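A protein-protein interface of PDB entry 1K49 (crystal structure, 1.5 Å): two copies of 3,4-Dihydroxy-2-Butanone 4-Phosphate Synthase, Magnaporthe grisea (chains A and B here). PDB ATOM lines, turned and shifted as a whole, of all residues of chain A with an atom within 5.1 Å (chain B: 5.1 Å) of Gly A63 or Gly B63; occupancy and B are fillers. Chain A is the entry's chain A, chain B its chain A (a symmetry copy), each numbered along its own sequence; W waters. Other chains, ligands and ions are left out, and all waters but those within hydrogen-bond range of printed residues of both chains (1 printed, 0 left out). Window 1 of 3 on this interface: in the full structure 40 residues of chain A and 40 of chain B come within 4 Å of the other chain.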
ATOM      1  N   MET A  57      25.562  -7.355  16.194  1.00  0.00           N
ATOM      2  CA  MET A  57      24.181  -7.209  15.689  1.00  0.00           C
ATOM      3  C   MET A  57      23.475  -8.546  15.656  1.00  0.00           C
ATOM      4  O   MET A  57      22.306  -8.693  16.093  1.00  0.00           O
ATOM      5  CB  MET A  57      24.220  -6.669  14.252  1.00  0.00           C
ATOM      6  CG  MET A  57      22.891  -6.011  13.879  1.00  0.00           C
ATOM      7  SD  MET A  57      22.947  -5.259  12.212  1.00  0.00           S
ATOM      8  CE  MET A  57      21.583  -4.078  12.354  1.00  0.00           C
ATOM      9  N   VAL A  58      24.241  -9.519  15.184  1.00  0.00           N
ATOM     10  CA  VAL A  58      23.673 -10.871  15.101  1.00  0.00           C
ATOM     11  C   VAL A  58      23.336 -11.398  16.489  1.00  0.00           C
ATOM     12  O   VAL A  58      22.223 -11.888  16.782  1.00  0.00           O
ATOM     13  CB  VAL A  58      24.613 -11.799  14.375  1.00  0.00           C
ATOM     14  CG1 VAL A  58      24.117 -13.237  14.471  1.00  0.00           C
ATOM     15  CG2 VAL A  58      24.624 -11.388  12.881  1.00  0.00           C
ATOM     16  N   SER A  61      20.160  -9.593  18.128  1.00  0.00           N
ATOM     17  CA  SER A  61      18.926  -9.301  17.387  1.00  0.00           C
ATOM     18  C   SER A  61      18.336 -10.622  16.922  1.00  0.00           C
ATOM     19  O   SER A  61      18.913 -11.664  17.257  1.00  0.00           O
ATOM     20  CB  SER A  61      19.172  -8.439  16.151  1.00  0.00           C
ATOM     21  OG  SER A  61      19.923  -9.161  15.171  1.00  0.00           O
ATOM     22  N   SER A  62      17.272 -10.543  16.088  1.00  0.00           N
ATOM     23  CA  SER A  62      16.693 -11.768  15.491  1.00  0.00           C
ATOM     24  C   SER A  62      17.694 -12.519  14.619  1.00  0.00           C
ATOM     25  O   SER A  62      17.535 -13.728  14.304  1.00  0.00           O
ATOM     26  CB  SER A  62      15.533 -11.352  14.583  1.00  0.00           C
ATOM     27  OG  SER A  62      16.104 -10.651  13.469  1.00  0.00           O
ATOM     28  N   GLY A  63      18.783 -11.809  14.187  1.00  0.00           N
ATOM     29  CA  GLY A  63      19.742 -12.422  13.274  1.00  0.00           C
ATOM     30  C   GLY A  63      19.242 -12.310  11.791  1.00  0.00           C
ATOM     31  O   GLY A  63      19.978 -12.706  10.875  1.00  0.00           O
ATOM     32  N   LEU A  64      17.996 -11.837  11.543  1.00  0.00           N
ATOM     33  CA  LEU A  64      17.571 -11.628  10.158  1.00  0.00           C
ATOM     34  C   LEU A  64      18.041 -10.181   9.824  1.00  0.00           C
ATOM     35  O   LEU A  64      17.402  -9.176  10.123  1.00  0.00           O
ATOM     36  CB  LEU A  64      16.069 -11.775  10.003  1.00  0.00           C
ATOM     37  CG  LEU A  64      15.581 -11.619   8.568  1.00  0.00           C
ATOM     38  CD1 LEU A  64      16.158 -12.725   7.699  1.00  0.00           C
ATOM     39  CD2 LEU A  64      14.078 -11.827   8.609  1.00  0.00           C
ATOM     40  N   ILE A  65      19.259 -10.152   9.269  1.00  0.00           N
ATOM     41  CA  ILE A  65      19.984  -8.915   8.942  1.00  0.00           C
ATOM     42  C   ILE A  65      19.547  -8.420   7.552  1.00  0.00           C
ATOM     43  O   ILE A  65      19.795  -9.136   6.547  1.00  0.00           O
ATOM     44  CB  ILE A  65      21.503  -9.142   9.007  1.00  0.00           C
ATOM     45  CG1 ILE A  65      21.931  -9.766  10.348  1.00  0.00           C
ATOM     46  CG2 ILE A  65      22.208  -7.789   8.767  1.00  0.00           C
ATOM     47  CD1 ILE A  65      21.518  -8.957  11.583  1.00  0.00           C
ATOM     48  N   ARG A 114      28.444 -11.304   6.001  1.00  0.00           N
ATOM     49  CA  ARG A 114      27.271 -10.466   5.950  1.00  0.00           C
ATOM     50  C   ARG A 114      27.647  -8.976   6.008  1.00  0.00           C
ATOM     51  O   ARG A 114      27.025  -8.115   5.335  1.00  0.00           O
ATOM     52  CB  ARG A 114      26.144 -10.868   6.935  1.00  0.00           C
ATOM     53  CG  ARG A 114      25.584 -12.273   6.594  1.00  0.00           C
ATOM     54  CD  ARG A 114      24.279 -12.551   7.354  1.00  0.00           C
ATOM     55  NE  ARG A 114      24.516 -13.131   8.694  1.00  0.00           N
ATOM     56  CZ  ARG A 114      23.500 -13.403   9.521  1.00  0.00           C
ATOM     57  NH1 ARG A 114      22.218 -13.133   9.196  1.00  0.00           N
ATOM     58  NH2 ARG A 114      23.761 -13.975  10.701  1.00  0.00           N
ATOM     59  N   SER A 173      17.896  -4.658  12.025  1.00  0.00           N
ATOM     60  CA  SER A 173      17.519  -5.958  12.555  1.00  0.00           C
ATOM     61  C   SER A 173      16.679  -5.712  13.804  1.00  0.00           C
ATOM     62  O   SER A 173      16.950  -4.744  14.528  1.00  0.00           O
ATOM     63  CB  SER A 173      18.685  -6.901  12.816  1.00  0.00           C
ATOM     64  OG  SER A 173      18.091  -8.190  12.840  1.00  0.00           O
ATOM     65  N   MET B  57      17.378 -21.527  19.490  1.00  0.00           N
ATOM     66  CA  MET B  57      17.974 -21.650  18.144  1.00  0.00           C
ATOM     67  C   MET B  57      18.454 -20.307  17.641  1.00  0.00           C
ATOM     68  O   MET B  57      19.582 -20.158  17.108  1.00  0.00           O
ATOM     69  CB  MET B  57      16.910 -22.161  17.162  1.00  0.00           C
ATOM     70  CG  MET B  57      17.562 -22.800  15.934  1.00  0.00           C
ATOM     71  SD  MET B  57      16.319 -23.517  14.800  1.00  0.00           S
ATOM     72  CE  MET B  57      17.359 -24.689  13.894  1.00  0.00           C
ATOM     73  N   VAL B  58      17.591 -19.331  17.883  1.00  0.00           N
ATOM     74  CA  VAL B  58      17.938 -17.972  17.445  1.00  0.00           C
ATOM     75  C   VAL B  58      19.174 -17.471  18.179  1.00  0.00           C
ATOM     76  O   VAL B  58      20.163 -16.978  17.594  1.00  0.00           O
ATOM     77  CB  VAL B  58      16.771 -17.038  17.635  1.00  0.00           C
ATOM     78  CG1 VAL B  58      17.197 -15.598  17.375  1.00  0.00           C
ATOM     79  CG2 VAL B  58      15.686 -17.418  16.595  1.00  0.00           C
ATOM     80  N   SER B  61      22.545 -19.282  17.001  1.00  0.00           N
ATOM     81  CA  SER B  61      22.869 -19.548  15.593  1.00  0.00           C
ATOM     82  C   SER B  61      22.956 -18.213  14.873  1.00  0.00           C
ATOM     83  O   SER B  61      22.804 -17.182  15.541  1.00  0.00           O
ATOM     84  CB  SER B  61      21.802 -20.386  14.892  1.00  0.00           C
ATOM     85  OG  SER B  61      20.582 -19.651  14.765  1.00  0.00           O
ATOM     86  N   SER B  62      23.097 -18.265  13.526  1.00  0.00           N
ATOM     87  CA  SER B  62      23.081 -17.024  12.721  1.00  0.00           C
ATOM     88  C   SER B  62      21.765 -16.263  12.849  1.00  0.00           C
ATOM     89  O   SER B  62      21.661 -15.047  12.540  1.00  0.00           O
ATOM     90  CB  SER B  62      23.233 -17.411  11.247  1.00  0.00           C
ATOM     91  OG  SER B  62      22.029 -18.093  10.869  1.00  0.00           O
ATOM     92  N   GLY B  63      20.691 -16.974  13.316  1.00  0.00           N
ATOM     93  CA  GLY B  63      19.373 -16.350  13.383  1.00  0.00           C
ATOM     94  C   GLY B  63      18.655 -16.427  11.990  1.00  0.00           C
ATOM     95  O   GLY B  63      17.488 -16.019  11.889  1.00  0.00           O
ATOM     96  N   LEU B  64      19.340 -16.885  10.913  1.00  0.00           N
ATOM     97  CA  LEU B  64      18.638 -17.062   9.640  1.00  0.00           C
ATOM     98  C   LEU B  64      18.059 -18.505   9.716  1.00  0.00           C
ATOM     99  O   LEU B  64      18.710 -19.511   9.444  1.00  0.00           O
ATOM    100  CB  LEU B  64      19.573 -16.898   8.456  1.00  0.00           C
ATOM    101  CG  LEU B  64      18.880 -17.021   7.105  1.00  0.00           C
ATOM    102  CD1 LEU B  64      17.865 -15.902   6.937  1.00  0.00           C
ATOM    103  CD2 LEU B  64      19.958 -16.800   6.058  1.00  0.00           C
ATOM    104  N   ILE B  65      16.813 -18.534  10.204  1.00  0.00           N
ATOM    105  CA  ILE B  65      16.063 -19.770  10.472  1.00  0.00           C
ATOM    106  C   ILE B  65      15.364 -20.233   9.181  1.00  0.00           C
ATOM    107  O   ILE B  65      14.476 -19.499   8.675  1.00  0.00           O
ATOM    108  CB  ILE B  65      15.055 -19.558  11.613  1.00  0.00           C
ATOM    109  CG1 ILE B  65      15.726 -18.965  12.866  1.00  0.00           C
ATOM    110  CG2 ILE B  65      14.380 -20.911  11.925  1.00  0.00           C
ATOM    111  CD1 ILE B  65      16.893 -19.796  13.411  1.00  0.00           C
ATOM    112  N   ARG B 114       8.086 -17.394  14.553  1.00  0.00           N
ATOM    113  CA  ARG B 114       8.858 -18.221  13.658  1.00  0.00           C
ATOM    114  C   ARG B 114       8.625 -19.716  13.937  1.00  0.00           C
ATOM    115  O   ARG B 114       8.567 -20.557  13.005  1.00  0.00           O
ATOM    116  CB  ARG B 114      10.353 -17.830  13.542  1.00  0.00           C
ATOM    117  CG  ARG B 114      10.510 -16.413  12.931  1.00  0.00           C
ATOM    118  CD  ARG B 114      11.966 -16.140  12.528  1.00  0.00           C
ATOM    119  NE  ARG B 114      12.769 -15.589  13.641  1.00  0.00           N
ATOM    120  CZ  ARG B 114      14.072 -15.325  13.493  1.00  0.00           C
ATOM    121  NH1 ARG B 114      14.728 -15.578  12.340  1.00  0.00           N
ATOM    122  NH2 ARG B 114      14.743 -14.780  14.512  1.00  0.00           N
ATOM    123  N   SER B 173      19.693 -24.071  11.029  1.00  0.00           N
ATOM    124  CA  SER B 173      20.347 -22.779  11.154  1.00  0.00           C
ATOM    125  C   SER B 173      21.827 -23.043  11.414  1.00  0.00           C
ATOM    126  O   SER B 173      22.150 -24.028  12.092  1.00  0.00           O
ATOM    127  CB  SER B 173      19.732 -21.851  12.191  1.00  0.00           C
ATOM    128  OG  SER B 173      20.173 -20.558  11.808  1.00  0.00           O
HETATM  129  O   HOH W   1      21.404 -14.439  17.687  1.00  0.00           O
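O of Ser B62 sits close to O of Gly A63, 3.3 Å away. O of Ser A62 lies close to O of Gly B63 (3.3 Å). O of Ser A62 lies within hydrogen-bond range of NH2 of Arg B114, 3.0 Å away. NH2 of Arg A114 is in hydrogen-bond range of O of Ser B62.
Water W1 bridges the backbone carbonyl oxygen of Val A58 (2.8 Å) and the backbone carbonyl oxygen of Val B58 (2.8 Å).
The guanidinium group of Arg B114 is in hydrogen-bond range of the backbone carbonyl oxygen of Gly B63 (2.8 Å). The backbone carbonyl oxygen (O) of Leu A64 sits at hydrogen-bond distance from the side-chain hydroxyl (OG) of Ser A173 (3.0 Å). The side-chain hydroxyl (OG) of Ser B62 sits at hydrogen-bond distance from the backbone NH (N) of Leu B64 (2.9 Å). The side-chain hydroxyl (OG) of Ser A62 is in hydrogen-bond range of the backbone NH (N) of Leu A64. The side-chain hydroxyl of Ser A62 is in hydrogen-bond range of the side-chain hydroxyl of Ser A173. O of Gly A63 is in hydrogen-bond range of NH1 of Arg A114 (2.8 Å).
Gly A63 touches two residues of chain B. Of chain A, only Ser A62 (3.3 Å) and Gly A63 (3.9 Å) come within 4 Å of Gly B63. Of the printed residues of chain B, Arg A114 touches Ser B62. Of the printed residues of chain B, Ser A62 touches Val B58, Gly B63 and Arg B114. The nearest residue of chain A that does not touch Gly B63 is Leu A64 (4.2 Å). The nearest printed residue of chain A that does not touch Leu B64 is Gly A63 (4.2 Å).
Ser A62 touches Gly B63, and with the chains exchanged Gly A63 touches Ser B62. Ser A62 touches Arg B114, and with the chains exchanged Arg A114 touches Ser B62. Gly B63 touches its own counterpart, Gly A63. Leu B64 touches its own counterpart, Leu A64. Positions printed for both chains: 57, 58, 61, 62, 63, 64, 65, 114 and 173.
Hydrophobic or aromatic side chains of chain A within 4 Å of the printed part of chain B: Val A58 and Leu A64. Of the 9 printed residues of chain B, 5 touch a printed residue of chain A. Hydrophobic or aromatic side chains of chain B within 4 Å of the printed part of chain A: Val B58 and Leu B64. Among the printed residues, 8 pairs touch across the chains. Among the printed residues, no Asp or Glu carboxylate lies within 4 Å of a Lys or Arg side-chain nitrogen of the other chain.
CG1 of Val A58 touches O of Ser B62, 3.6 Å away. Val B58 touches Ser A62 (CG1 to O, 3.6 Å). Gly B63 touches Gly A63. Leu A64 touches Leu B64 (CD1 to CD1, 3.7 Å).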
